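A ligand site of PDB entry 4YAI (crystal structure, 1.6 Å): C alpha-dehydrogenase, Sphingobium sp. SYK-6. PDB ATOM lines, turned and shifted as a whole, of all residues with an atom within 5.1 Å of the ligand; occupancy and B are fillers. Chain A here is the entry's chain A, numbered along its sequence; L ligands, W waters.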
ATOM      1  N   GLY A  12      -0.577 -22.594  -7.644  1.00  0.00           N
ATOM      2  CA  GLY A  12       0.408 -21.732  -8.289  1.00  0.00           C
ATOM      3  C   GLY A  12      -0.167 -21.060  -9.520  1.00  0.00           C
ATOM      4  O   GLY A  12       0.570 -20.735 -10.452  1.00  0.00           O
ATOM      5  N   ALA A  14      -1.327 -18.141 -10.064  1.00  0.00           N
ATOM      6  CA  ALA A  14      -1.203 -16.673 -10.134  1.00  0.00           C
ATOM      7  C   ALA A  14       0.144 -16.199 -10.687  1.00  0.00           C
ATOM      8  O   ALA A  14       0.422 -15.007 -10.694  1.00  0.00           O
ATOM      9  CB  ALA A  14      -1.447 -16.069  -8.762  1.00  0.00           C
ATOM     10  N   SER A  15       0.974 -17.136 -11.135  1.00  0.00           N
ATOM     11  CA  SER A  15       2.267 -16.787 -11.704  1.00  0.00           C
ATOM     12  C   SER A  15       2.742 -17.869 -12.669  1.00  0.00           C
ATOM     13  O   SER A  15       2.273 -19.010 -12.621  1.00  0.00           O
ATOM     14  CB  SER A  15       3.313 -16.594 -10.609  1.00  0.00           C
ATOM     15  OG  SER A  15       4.542 -16.124 -11.148  1.00  0.00           O
ATOM     16  N   GLY A  16       3.664 -17.496 -13.556  1.00  0.00           N
ATOM     17  CA  GLY A  16       4.402 -18.452 -14.356  1.00  0.00           C
ATOM     18  C   GLY A  16       3.558 -19.441 -15.145  1.00  0.00           C
ATOM     19  O   GLY A  16       2.589 -19.084 -15.810  1.00  0.00           O
ATOM     20  N   ILE A  17       3.974 -20.707 -15.107  1.00  0.00           N
ATOM     21  CA  ILE A  17       3.296 -21.756 -15.859  1.00  0.00           C
ATOM     22  C   ILE A  17       1.827 -21.869 -15.503  1.00  0.00           C
ATOM     23  O   ILE A  17       0.966 -22.009 -16.371  1.00  0.00           O
ATOM     24  CB  ILE A  17       3.975 -23.110 -15.636  1.00  0.00           C
ATOM     25  CG1 ILE A  17       5.361 -23.064 -16.267  1.00  0.00           C
ATOM     26  CG2 ILE A  17       3.137 -24.249 -16.201  1.00  0.00           C
ATOM     27  CD1 ILE A  17       6.255 -24.248 -15.925  1.00  0.00           C
ATOM     28  N   GLY A  18       1.529 -21.820 -14.207  1.00  0.00           N
ATOM     29  CA  GLY A  18       0.159 -21.928 -13.742  1.00  0.00           C
ATOM     30  C   GLY A  18      -0.724 -20.831 -14.311  1.00  0.00           C
ATOM     31  O   GLY A  18      -1.876 -21.069 -14.670  1.00  0.00           O
ATOM     32  N   ALA A  35      -5.228 -20.864  -6.780  1.00  0.00           N
ATOM     33  CA  ALA A  35      -4.756 -21.061  -5.416  1.00  0.00           C
ATOM     34  C   ALA A  35      -3.251 -20.801  -5.345  1.00  0.00           C
ATOM     35  O   ALA A  35      -2.467 -21.403  -6.098  1.00  0.00           O
ATOM     36  CB  ALA A  35      -5.094 -22.474  -4.936  1.00  0.00           C
ATOM     37  N   ASP A  36      -2.839 -19.931  -4.438  1.00  0.00           N
ATOM     38  CA  ASP A  36      -1.446 -19.480  -4.400  1.00  0.00           C
ATOM     39  C   ASP A  36      -1.105 -18.984  -3.006  1.00  0.00           C
ATOM     40  O   ASP A  36      -1.975 -18.478  -2.308  1.00  0.00           O
ATOM     41  CB  ASP A  36      -1.247 -18.369  -5.442  1.00  0.00           C
ATOM     42  CG  ASP A  36       0.183 -18.259  -5.918  1.00  0.00           C
ATOM     43  OD1 ASP A  36       1.046 -17.826  -5.115  1.00  0.00           O
ATOM     44  OD2 ASP A  36       0.446 -18.609  -7.095  1.00  0.00           O
ATOM     45  N   ILE A  37       0.162 -19.123  -2.622  1.00  0.00           N
ATOM     46  CA  ILE A  37       0.597 -18.722  -1.296  1.00  0.00           C
ATOM     47  C   ILE A  37       0.936 -17.226  -1.252  1.00  0.00           C
ATOM     48  O   ILE A  37       1.057 -16.643  -0.167  1.00  0.00           O
ATOM     49  CB  ILE A  37       1.833 -19.578  -0.852  1.00  0.00           C
ATOM     50  CG1 ILE A  37       2.000 -19.552   0.665  1.00  0.00           C
ATOM     51  CG2 ILE A  37       3.104 -19.131  -1.609  1.00  0.00           C
ATOM     52  CD1 ILE A  37       3.002 -20.556   1.204  1.00  0.00           C
ATOM     53  N   ARG A  38       1.067 -16.601  -2.421  1.00  0.00           N
ATOM     54  CA  ARG A  38       1.488 -15.203  -2.534  1.00  0.00           C
ATOM     55  C   ARG A  38       0.304 -14.300  -2.818  1.00  0.00           C
ATOM     56  O   ARG A  38      -0.250 -14.319  -3.923  1.00  0.00           O
ATOM     57  CB  ARG A  38       2.546 -15.062  -3.632  1.00  0.00           C
ATOM     58  CG  ARG A  38       3.924 -15.597  -3.263  1.00  0.00           C
ATOM     59  CD  ARG A  38       4.726 -14.613  -2.434  1.00  0.00           C
ATOM     60  NE  ARG A  38       5.012 -13.388  -3.177  1.00  0.00           N
ATOM     61  CZ  ARG A  38       5.999 -13.237  -4.053  1.00  0.00           C
ATOM     62  NH1 ARG A  38       6.857 -14.229  -4.298  1.00  0.00           N
ATOM     63  NH2 ARG A  38       6.150 -12.079  -4.669  1.00  0.00           N
ATOM     64  N   HIS A  41       0.803 -11.953  -5.837  1.00  0.00           N
ATOM     65  CA  HIS A  41       0.595 -12.656  -7.102  1.00  0.00           C
ATOM     66  C   HIS A  41      -0.898 -12.794  -7.406  1.00  0.00           C
ATOM     67  O   HIS A  41      -1.336 -12.554  -8.530  1.00  0.00           O
ATOM     68  CB  HIS A  41       1.239 -14.050  -7.078  1.00  0.00           C
ATOM     69  CG  HIS A  41       2.735 -14.028  -7.138  1.00  0.00           C
ATOM     70  ND1 HIS A  41       3.494 -15.171  -7.250  1.00  0.00           N
ATOM     71  CD2 HIS A  41       3.610 -12.992  -7.111  1.00  0.00           C
ATOM     72  CE1 HIS A  41       4.769 -14.853  -7.292  1.00  0.00           C
ATOM     73  NE2 HIS A  41       4.873 -13.539  -7.211  1.00  0.00           N
ATOM     74  N   LEU A  63      -3.487 -19.930  -0.156  1.00  0.00           N
ATOM     75  CA  LEU A  63      -3.239 -21.118   0.626  1.00  0.00           C
ATOM     76  C   LEU A  63      -1.853 -21.670   0.377  1.00  0.00           C
ATOM     77  O   LEU A  63      -1.154 -21.264  -0.541  1.00  0.00           O
ATOM     78  CB  LEU A  63      -4.275 -22.204   0.315  1.00  0.00           C
ATOM     79  CG  LEU A  63      -4.427 -22.677  -1.135  1.00  0.00           C
ATOM     80  CD1 LEU A  63      -3.290 -23.567  -1.602  1.00  0.00           C
ATOM     81  CD2 LEU A  63      -5.753 -23.419  -1.299  1.00  0.00           C
ATOM     82  N   ASP A  64      -1.471 -22.581   1.262  1.00  0.00           N
ATOM     83  CA  ASP A  64      -0.239 -23.354   1.193  1.00  0.00           C
ATOM     84  C   ASP A  64      -0.634 -24.792   0.861  1.00  0.00           C
ATOM     85  O   ASP A  64      -1.339 -25.422   1.647  1.00  0.00           O
ATOM     86  CB  ASP A  64       0.484 -23.254   2.526  1.00  0.00           C
ATOM     87  CG  ASP A  64       1.742 -24.121   2.613  1.00  0.00           C
ATOM     88  OD1 ASP A  64       2.084 -24.847   1.653  1.00  0.00           O
ATOM     89  OD2 ASP A  64       2.381 -24.050   3.685  1.00  0.00           O
ATOM     90  N   VAL A  65      -0.201 -25.286  -0.293  1.00  0.00           N
ATOM     91  CA  VAL A  65      -0.618 -26.620  -0.728  1.00  0.00           C
ATOM     92  C   VAL A  65      -0.138 -27.723   0.206  1.00  0.00           C
ATOM     93  O   VAL A  65      -0.642 -28.854   0.133  1.00  0.00           O
ATOM     94  CB  VAL A  65      -0.114 -26.956  -2.156  1.00  0.00           C
ATOM     95  CG1 VAL A  65      -0.766 -26.027  -3.183  1.00  0.00           C
ATOM     96  CG2 VAL A  65       1.401 -26.912  -2.247  1.00  0.00           C
ATOM     97  N   SER A  66       0.825 -27.437   1.083  1.00  0.00           N
ATOM     98  CA  SER A  66       1.300 -28.449   2.020  1.00  0.00           C
ATOM     99  C   SER A  66       0.545 -28.419   3.353  1.00  0.00           C
ATOM    100  O   SER A  66       0.897 -29.129   4.287  1.00  0.00           O
ATOM    101  CB  SER A  66       2.809 -28.290   2.261  1.00  0.00           C
ATOM    102  OG  SER A  66       3.136 -27.033   2.862  1.00  0.00           O
ATOM    103  N   ASN A  91       0.193 -27.640  -9.702  1.00  0.00           N
ATOM    104  CA  ASN A  91       1.289 -27.006 -10.415  1.00  0.00           C
ATOM    105  C   ASN A  91       2.278 -26.251  -9.531  1.00  0.00           C
ATOM    106  O   ASN A  91       3.438 -26.076  -9.921  1.00  0.00           O
ATOM    107  CB  ASN A  91       0.711 -26.067 -11.482  1.00  0.00           C
ATOM    108  CG  ASN A  91       1.713 -25.051 -11.977  1.00  0.00           C
ATOM    109  OD1 ASN A  91       2.505 -25.331 -12.884  1.00  0.00           O
ATOM    110  ND2 ASN A  91       1.688 -23.874 -11.388  1.00  0.00           N
ATOM    111  N   ALA A  92       1.845 -25.808  -8.356  1.00  0.00           N
ATOM    112  CA  ALA A  92       2.727 -25.048  -7.479  1.00  0.00           C
ATOM    113  C   ALA A  92       4.038 -25.802  -7.243  1.00  0.00           C
ATOM    114  O   ALA A  92       4.044 -27.025  -7.120  1.00  0.00           O
ATOM    115  CB  ALA A  92       2.041 -24.743  -6.152  1.00  0.00           C
ATOM    116  N   GLY A  93       5.140 -25.070  -7.198  1.00  0.00           N
ATOM    117  CA  GLY A  93       6.417 -25.673  -6.885  1.00  0.00           C
ATOM    118  C   GLY A  93       7.389 -24.594  -6.541  1.00  0.00           C
ATOM    119  O   GLY A  93       7.155 -23.412  -6.834  1.00  0.00           O
ATOM    120  N   ILE A  94       8.492 -24.999  -5.928  1.00  0.00           N
ATOM    121  CA  ILE A  94       9.555 -24.083  -5.575  1.00  0.00           C
ATOM    122  C   ILE A  94      10.900 -24.717  -5.900  1.00  0.00           C
ATOM    123  O   ILE A  94      10.981 -25.906  -6.208  1.00  0.00           O
ATOM    124  CB  ILE A  94       9.484 -23.668  -4.085  1.00  0.00           C
ATOM    125  CG1 ILE A  94       9.186 -24.861  -3.170  1.00  0.00           C
ATOM    126  CG2 ILE A  94       8.410 -22.603  -3.897  1.00  0.00           C
ATOM    127  CD1 ILE A  94      10.361 -25.794  -2.928  1.00  0.00           C
ATOM    128  N   ILE A 114       6.357 -29.259  -0.574  1.00  0.00           N
ATOM    129  CA  ILE A 114       5.707 -28.474  -1.616  1.00  0.00           C
ATOM    130  C   ILE A 114       5.637 -29.261  -2.914  1.00  0.00           C
ATOM    131  O   ILE A 114       4.575 -29.368  -3.514  1.00  0.00           O
ATOM    132  CB  ILE A 114       6.406 -27.126  -1.882  1.00  0.00           C
ATOM    133  CG1 ILE A 114       6.656 -26.367  -0.580  1.00  0.00           C
ATOM    134  CG2 ILE A 114       5.602 -26.301  -2.867  1.00  0.00           C
ATOM    135  CD1 ILE A 114       5.443 -26.272   0.311  1.00  0.00           C
ATOM    136  N   ASN A 115       6.762 -29.816  -3.341  1.00  0.00           N
ATOM    137  CA  ASN A 115       6.841 -30.365  -4.696  1.00  0.00           C
ATOM    138  C   ASN A 115       6.294 -31.807  -4.833  1.00  0.00           C
ATOM    139  O   ASN A 115       5.927 -32.215  -5.940  1.00  0.00           O
ATOM    140  CB  ASN A 115       8.299 -30.289  -5.210  1.00  0.00           C
ATOM    141  CG  ASN A 115       8.738 -28.859  -5.517  1.00  0.00           C
ATOM    142  OD1 ASN A 115       7.935 -27.919  -5.523  1.00  0.00           O
ATOM    143  ND2 ASN A 115      10.032 -28.664  -5.735  1.00  0.00           N
ATOM    144  N   THR A 142       2.438 -30.821 -12.408  1.00  0.00           N
ATOM    145  CA  THR A 142       3.634 -30.255 -12.988  1.00  0.00           C
ATOM    146  C   THR A 142       4.864 -30.831 -12.308  1.00  0.00           C
ATOM    147  O   THR A 142       5.148 -30.504 -11.150  1.00  0.00           O
ATOM    148  CB  THR A 142       3.697 -28.717 -12.877  1.00  0.00           C
ATOM    149  OG1 THR A 142       2.492 -28.152 -13.394  1.00  0.00           O
ATOM    150  CG2 THR A 142       4.883 -28.194 -13.699  1.00  0.00           C
ATOM    151  N   ALA A 143       5.571 -31.681 -13.031  1.00  0.00           N
ATOM    152  CA  ALA A 143       6.858 -32.195 -12.580  1.00  0.00           C
ATOM    153  C   ALA A 143       7.958 -31.308 -13.178  1.00  0.00           C
ATOM    154  O   ALA A 143       7.914 -30.097 -13.022  1.00  0.00           O
ATOM    155  CB  ALA A 143       7.027 -33.651 -12.969  1.00  0.00           C
ATOM    156  N   SER A 144       8.915 -31.925 -13.878  1.00  0.00           N
ATOM    157  CA  SER A 144      10.015 -31.226 -14.516  1.00  0.00           C
ATOM    158  C   SER A 144      10.804 -32.229 -15.322  1.00  0.00           C
ATOM    159  O   SER A 144      10.822 -33.403 -14.977  1.00  0.00           O
ATOM    160  CB  SER A 144      10.951 -30.557 -13.506  1.00  0.00           C
ATOM    161  OG  SER A 144      12.071 -29.971 -14.159  1.00  0.00           O
ATOM    162  N   LEU A 145      11.485 -31.774 -16.373  1.00  0.00           N
ATOM    163  CA  LEU A 145      12.435 -32.646 -17.028  1.00  0.00           C
ATOM    164  C   LEU A 145      13.600 -32.973 -16.084  1.00  0.00           C
ATOM    165  O   LEU A 145      14.302 -33.956 -16.289  1.00  0.00           O
ATOM    166  CB  LEU A 145      12.943 -32.027 -18.332  1.00  0.00           C
ATOM    167  CG  LEU A 145      11.926 -32.106 -19.471  1.00  0.00           C
ATOM    168  CD1 LEU A 145      12.317 -31.215 -20.641  1.00  0.00           C
ATOM    169  CD2 LEU A 145      11.743 -33.542 -19.955  1.00  0.00           C
ATOM    170  N   TYR A 158      15.106 -31.094  -5.404  1.00  0.00           N
ATOM    171  CA  TYR A 158      14.200 -30.804  -6.508  1.00  0.00           C
ATOM    172  C   TYR A 158      14.000 -32.034  -7.403  1.00  0.00           C
ATOM    173  O   TYR A 158      12.881 -32.455  -7.663  1.00  0.00           O
ATOM    174  CB  TYR A 158      14.727 -29.641  -7.326  1.00  0.00           C
ATOM    175  CG  TYR A 158      13.773 -29.091  -8.356  1.00  0.00           C
ATOM    176  CD1 TYR A 158      12.758 -28.205  -7.996  1.00  0.00           C
ATOM    177  CD2 TYR A 158      13.901 -29.424  -9.691  1.00  0.00           C
ATOM    178  CE1 TYR A 158      11.888 -27.691  -8.946  1.00  0.00           C
ATOM    179  CE2 TYR A 158      13.047 -28.894 -10.650  1.00  0.00           C
ATOM    180  CZ  TYR A 158      12.041 -28.031 -10.271  1.00  0.00           C
ATOM    181  OH  TYR A 158      11.199 -27.505 -11.224  1.00  0.00           O
ATOM    182  N   LYS A 162      10.553 -34.283  -8.084  1.00  0.00           N
ATOM    183  CA  LYS A 162       9.969 -34.256  -9.413  1.00  0.00           C
ATOM    184  C   LYS A 162       9.906 -35.647 -10.058  1.00  0.00           C
ATOM    185  O   LYS A 162       8.940 -35.942 -10.761  1.00  0.00           O
ATOM    186  CB  LYS A 162      10.732 -33.272 -10.298  1.00  0.00           C
ATOM    187  CG  LYS A 162      10.581 -31.818  -9.838  1.00  0.00           C
ATOM    188  CD  LYS A 162       9.131 -31.358  -9.830  1.00  0.00           C
ATOM    189  CE  LYS A 162       8.983 -29.857  -9.732  1.00  0.00           C
ATOM    190  NZ  LYS A 162       7.570 -29.420  -9.869  1.00  0.00           N
ATOM    191  N   PRO A 188       8.352 -29.639 -17.797  1.00  0.00           N
ATOM    192  CA  PRO A 188       8.943 -28.521 -18.530  1.00  0.00           C
ATOM    193  C   PRO A 188      10.467 -28.458 -18.513  1.00  0.00           C
ATOM    194  O   PRO A 188      11.121 -28.970 -17.596  1.00  0.00           O
ATOM    195  CB  PRO A 188       8.373 -27.284 -17.821  1.00  0.00           C
ATOM    196  CG  PRO A 188       7.230 -27.789 -16.976  1.00  0.00           C
ATOM    197  CD  PRO A 188       7.630 -29.175 -16.598  1.00  0.00           C
ATOM    198  N   GLY A 189      10.984 -27.838 -19.567  1.00  0.00           N
ATOM    199  CA  GLY A 189      12.307 -27.249 -19.568  1.00  0.00           C
ATOM    200  C   GLY A 189      12.158 -25.786 -19.184  1.00  0.00           C
ATOM    201  O   GLY A 189      11.186 -25.429 -18.537  1.00  0.00           O
ATOM    202  N   PRO A 190      13.097 -24.915 -19.609  1.00  0.00           N
ATOM    203  CA  PRO A 190      13.083 -23.513 -19.155  1.00  0.00           C
ATOM    204  C   PRO A 190      11.891 -22.690 -19.652  1.00  0.00           C
ATOM    205  O   PRO A 190      11.770 -22.455 -20.858  1.00  0.00           O
ATOM    206  CB  PRO A 190      14.399 -22.940 -19.716  1.00  0.00           C
ATOM    207  CG  PRO A 190      15.187 -24.119 -20.198  1.00  0.00           C
ATOM    208  CD  PRO A 190      14.221 -25.199 -20.518  1.00  0.00           C
ATOM    209  N   ILE A 191      11.026 -22.273 -18.721  1.00  0.00           N
ATOM    210  CA  ILE A 191       9.869 -21.439 -19.003  1.00  0.00           C
ATOM    211  C   ILE A 191      10.029 -20.111 -18.270  1.00  0.00           C
ATOM    212  O   ILE A 191      10.471 -20.097 -17.128  1.00  0.00           O
ATOM    213  CB  ILE A 191       8.551 -22.093 -18.536  1.00  0.00           C
ATOM    214  CG1 ILE A 191       8.486 -23.576 -18.916  1.00  0.00           C
ATOM    215  CG2 ILE A 191       7.336 -21.333 -19.083  1.00  0.00           C
ATOM    216  CD1 ILE A 191       8.624 -23.869 -20.384  1.00  0.00           C
ATOM    217  N   SER A 193       9.178 -17.430 -15.874  1.00  0.00           N
ATOM    218  CA  SER A 193       8.342 -17.449 -14.668  1.00  0.00           C
ATOM    219  C   SER A 193       8.996 -16.664 -13.542  1.00  0.00           C
ATOM    220  O   SER A 193       9.976 -15.956 -13.761  1.00  0.00           O
ATOM    221  CB  SER A 193       8.088 -18.877 -14.210  1.00  0.00           C
ATOM    222  OG  SER A 193       9.216 -19.381 -13.516  1.00  0.00           O
ATOM    223  N   ARG A 194       8.435 -16.796 -12.336  1.00  0.00           N
ATOM    224  CA  ARG A 194       8.967 -16.102 -11.171  1.00  0.00           C
ATOM    225  C   ARG A 194       9.442 -17.089 -10.099  1.00  0.00           C
ATOM    226  O   ARG A 194       9.485 -16.764  -8.917  1.00  0.00           O
ATOM    227  CB  ARG A 194       7.923 -15.131 -10.600  1.00  0.00           C
ATOM    228  CG  ARG A 194       7.713 -13.904 -11.484  1.00  0.00           C
ATOM    229  CD  ARG A 194       6.816 -12.849 -10.845  1.00  0.00           C
ATOM    230  NE  ARG A 194       5.402 -13.202 -10.974  1.00  0.00           N
ATOM    231  CZ  ARG A 194       4.401 -12.401 -10.614  1.00  0.00           C
ATOM    232  NH1 ARG A 194       4.646 -11.213 -10.094  1.00  0.00           N
ATOM    233  NH2 ARG A 194       3.140 -12.806 -10.766  1.00  0.00           N
ATOM    234  N   ILE A 195       9.840 -18.287 -10.531  1.00  0.00           N
ATOM    235  CA  ILE A 195      10.277 -19.316  -9.593  1.00  0.00           C
ATOM    236  C   ILE A 195      11.549 -18.872  -8.854  1.00  0.00           C
ATOM    237  O   ILE A 195      11.885 -19.421  -7.804  1.00  0.00           O
ATOM    238  CB  ILE A 195      10.496 -20.683 -10.294  1.00  0.00           C
ATOM    239  CG1 ILE A 195      10.645 -21.790  -9.249  1.00  0.00           C
ATOM    240  CG2 ILE A 195      11.700 -20.638 -11.236  1.00  0.00           C
ATOM    241  CD1 ILE A 195      10.458 -23.170  -9.799  1.00  0.00           C
ATOM    242  N   ASN A 201       8.615 -17.580  -1.160  1.00  0.00           N
ATOM    243  CA  ASN A 201       7.457 -18.461  -1.154  1.00  0.00           C
ATOM    244  C   ASN A 201       7.587 -19.585  -0.134  1.00  0.00           C
ATOM    245  O   ASN A 201       6.608 -20.282   0.148  1.00  0.00           O
ATOM    246  CB  ASN A 201       7.248 -19.046  -2.549  1.00  0.00           C
ATOM    247  CG  ASN A 201       7.088 -17.975  -3.613  1.00  0.00           C
ATOM    248  OD1 ASN A 201       6.777 -16.837  -3.300  1.00  0.00           O
ATOM    249  ND2 ASN A 201       7.315 -18.349  -4.873  1.00  0.00           N
ATOM    250  N   PRO A 203       7.243 -21.528   2.993  1.00  0.00           N
ATOM    251  CA  PRO A 203       6.381 -21.296   4.154  1.00  0.00           C
ATOM    252  C   PRO A 203       7.192 -21.008   5.407  1.00  0.00           C
ATOM    253  O   PRO A 203       8.333 -21.447   5.512  1.00  0.00           O
ATOM    254  CB  PRO A 203       5.586 -22.601   4.280  1.00  0.00           C
ATOM    255  CG  PRO A 203       5.615 -23.189   2.883  1.00  0.00           C
ATOM    256  CD  PRO A 203       6.973 -22.828   2.356  1.00  0.00           C
HETATM  257  P1  LIG L   1       6.285 -19.397 -10.387  1.00  0.00           P
HETATM  258  O1  LIG L   1       6.989 -19.057  -9.106  1.00  0.00           O
HETATM  259  O2  LIG L   1       6.230 -18.197 -11.363  1.00  0.00           O
HETATM  260  O3  LIG L   1       4.813 -19.875 -10.136  1.00  0.00           O
HETATM  261  C1  LIG L   1       4.580 -20.719  -9.048  1.00  0.00           C
HETATM  262  C2  LIG L   1       3.501 -20.194  -8.212  1.00  0.00           C
HETATM  263  O4  LIG L   1       3.290 -21.215  -7.191  1.00  0.00           O
HETATM  264  C3  LIG L   1       3.859 -18.942  -7.535  1.00  0.00           C
HETATM  265  O5  LIG L   1       2.875 -17.919  -7.717  1.00  0.00           O
HETATM  266  C4  LIG L   1       4.018 -19.288  -6.134  1.00  0.00           C
HETATM  267  O6  LIG L   1       3.644 -18.228  -5.237  1.00  0.00           O
HETATM  268  C5  LIG L   1       3.173 -20.461  -5.964  1.00  0.00           C
HETATM  269  N1  LIG L   1       3.547 -21.254  -4.834  1.00  0.00           N
HETATM  270  C6  LIG L   1       4.800 -21.595  -4.406  1.00  0.00           C
HETATM  271  N2  LIG L   1       4.717 -22.338  -3.305  1.00  0.00           N
HETATM  272  C7  LIG L   1       3.406 -22.519  -2.957  1.00  0.00           C
HETATM  273  C8  LIG L   1       2.699 -23.177  -1.952  1.00  0.00           C
HETATM  274  N3  LIG L   1       3.372 -23.858  -0.911  1.00  0.00           N
HETATM  275  N4  LIG L   1       1.337 -23.148  -1.930  1.00  0.00           N
HETATM  276  C9  LIG L   1       0.650 -22.501  -2.884  1.00  0.00           C
HETATM  277  N5  LIG L   1       1.288 -21.849  -3.879  1.00  0.00           N
HETATM  278  C10 LIG L   1       2.644 -21.827  -3.946  1.00  0.00           C
HETATM  279  O7  LIG L   1       7.167 -20.529 -11.028  1.00  0.00           O
HETATM  280  P2  LIG L   1       6.795 -21.623 -12.159  1.00  0.00           P
HETATM  281  O8  LIG L   1       5.619 -21.222 -13.045  1.00  0.00           O
HETATM  282  O9  LIG L   1       8.074 -21.809 -12.967  1.00  0.00           O
HETATM  283  O10 LIG L   1       6.469 -22.962 -11.323  1.00  0.00           O
HETATM  284  C11 LIG L   1       5.372 -23.800 -11.670  1.00  0.00           C
HETATM  285  C12 LIG L   1       5.802 -25.207 -11.654  1.00  0.00           C
HETATM  286  O11 LIG L   1       6.623 -25.451 -12.859  1.00  0.00           O
HETATM  287  C13 LIG L   1       6.627 -25.602 -10.505  1.00  0.00           C
HETATM  288  O12 LIG L   1       6.159 -26.874 -10.011  1.00  0.00           O
HETATM  289  C14 LIG L   1       7.986 -25.747 -11.013  1.00  0.00           C
HETATM  290  O13 LIG L   1       8.769 -26.654 -10.234  1.00  0.00           O
HETATM  291  C15 LIG L   1       7.764 -26.249 -12.353  1.00  0.00           C
HETATM  292  N6  LIG L   1       8.794 -26.102 -13.299  1.00  0.00           N
HETATM  293  C16 LIG L   1       9.151 -24.841 -13.744  1.00  0.00           C
HETATM  294  C17 LIG L   1      10.129 -24.717 -14.715  1.00  0.00           C
HETATM  295  C18 LIG L   1      10.539 -23.349 -15.193  1.00  0.00           C
HETATM  296  O14 LIG L   1       9.894 -22.310 -14.871  1.00  0.00           O
HETATM  297  N7  LIG L   1      11.744 -23.260 -16.046  1.00  0.00           N
HETATM  298  C19 LIG L   1      10.733 -25.840 -15.250  1.00  0.00           C
HETATM  299  C20 LIG L   1      10.343 -27.098 -14.819  1.00  0.00           C
HETATM  300  C21 LIG L   1       9.364 -27.216 -13.859  1.00  0.00           C
HETATM  301  O   HOH W   1      14.076 -24.492 -15.944  1.00  0.00           O
HETATM  302  O   HOH W   2      13.000 -27.637 -13.473  1.00  0.00           O
HETATM  303  O   HOH W   3       7.405 -20.637  -6.706  1.00  0.00           O
HETATM  304  O   HOH W   4       3.164 -21.439 -11.875  1.00  0.00           O
HETATM  305  O   HOH W   5       7.066 -16.958  -7.470  1.00  0.00           O
HETATM  306  O   HOH W   6       6.198 -22.777  -0.939  1.00  0.00           O
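Water W5 lies within hydrogen-bond range of an oxygen (O1) of the ligand, the backbone carbonyl oxygen (O) of Arg 194 and the side-chain amide nitrogen (ND2) of Asn 201.
Water W6 lies within hydrogen-bond range of O of Asn 201 (2.8 Å) and N2 of the ligand (2.8 Å).
Water W3 lies within hydrogen-bond range of O of Gly 93 (2.8 Å), O1 of the ligand (2.9 Å) and ND2 of Asn 201 (2.9 Å).
Water W2 bridges OG of Ser 144 (2.6 Å) and OH of Tyr 158 (2.9 Å).
A nitrogen (N4) of the ligand lies close to the backbone carbonyl oxygen (O) of Leu 63 (3.4 Å).
The backbone NH of Ile 191 sits close to a nitrogen (N7) of the ligand (2.9 Å).
CA of Gly 12 touches O4 of the ligand, 3.1 Å away.
Arg 38 touches the ligand (CG to O6, 3.3 Å).
O of Ala 92 touches O12 of the ligand, at 3.6 Å.
Ile 94 touches the ligand.
Ile 114 touches the ligand.
Thr 142 touches the ligand (CG2 to O11, 3.4 Å).
Ala 143 touches the ligand (O to C21, 3.3 Å).
OG of Ser 144 touches C20 of the ligand, 3.4 Å away.
Pro 188 touches the ligand.
CA of Pro 190 touches N7 of the ligand, at 3.4 Å.
ND2 of Asn 201 touches C4 of the ligand (3.7 Å).
29 residues have an atom within 4 Å of the ligand: Gly 12, Ser 15, Gly 16, Ile 17, Asp 36, Ile 37, Arg 38, His 41, Leu 63, Asp 64, Val 65, Asn 91, Ala 92, Gly 93, Ile 94, Ile 114, Thr 142, Ala 143, Ser 144, Tyr 158, Lys 162, Pro 188, Gly 189, Pro 190, Ile 191, Ser 193, Arg 194, Ile 195 and Asn 201.
Along chain A the residues within 4 Å of the ligand span positions 12 to 201.
OD2 of Asp 36 sits at hydrogen-bond distance from O5 of the ligand (2.6 Å).
The backbone NH of Ile 17 is in hydrogen-bond range of an oxygen (O8) of the ligand (2.7 Å).
The side-chain hydroxyl (OH) of Tyr 158 sits at hydrogen-bond distance from an oxygen (O13) of the ligand, 2.8 Å away.
O2 of the ligand sits at hydrogen-bond distance from N of Gly 16, at 3.4 Å.
The side-chain amino group (NZ) of Lys 162 sits at hydrogen-bond distance from an oxygen (O12) of the ligand, 2.9 Å away.
A nitrogen (N5) of the ligand lies within hydrogen-bond range of the backbone NH of Ile 37 (3.2 Å).
The side-chain hydroxyl (OG) of Ser 15 sits at hydrogen-bond distance from an oxygen (O2) of the ligand, at 2.7 Å.
The backbone NH of Ile 195 lies within hydrogen-bond range of an oxygen (O1) of the ligand (3.3 Å).
A nitrogen (N4) of the ligand is in hydrogen-bond range of the backbone NH of Val 65, at 3.1 Å.
The backbone NH (N) of Arg 194 is in hydrogen-bond range of an oxygen (O2) of the ligand, 2.8 Å away.
The backbone carbonyl oxygen (O) of Gly 189 sits close to a nitrogen (N7) of the ligand, 3.3 Å away.
The side-chain carboxylate of Asp 64 sits at hydrogen-bond distance from a nitrogen (N3) of the ligand, at 3.0 Å.
ND1 of His 41 sits at hydrogen-bond distance from O5 of the ligand.
OG of Ser 193 lies within hydrogen-bond range of O9 of the ligand.
O of Asn 91 is in hydrogen-bond range of O12 of the ligand (2.8 Å).
N of Gly 93 lies close to O12 of the ligand, 3.5 Å away.
N of Ile 37 lies close to O of Leu 63 (3.3 Å).
ND2 of Asn 115 is in hydrogen-bond range of O of Ile 94 (3.0 Å).
A ring nitrogen (NE2) of His 41 lies within hydrogen-bond range of the guanidinium group (NH2) of Arg 38, 3.2 Å away.
NH2 of Arg 194 sits at hydrogen-bond distance from O of Ala 14.
The backbone NH (N) of Leu 145 lies within hydrogen-bond range of the backbone carbonyl oxygen (O) of Pro 188.
N of Ala 14 is in hydrogen-bond range of OD2 of Asp 36 (3.5 Å).
The side-chain amide nitrogen (ND2) of Asn 91 lies close to the backbone NH (N) of Gly 18 (3.5 Å).
The backbone carbonyl oxygen (O) of Ala 35 is in hydrogen-bond range of the backbone NH (N) of Gly 12, at 2.7 Å.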
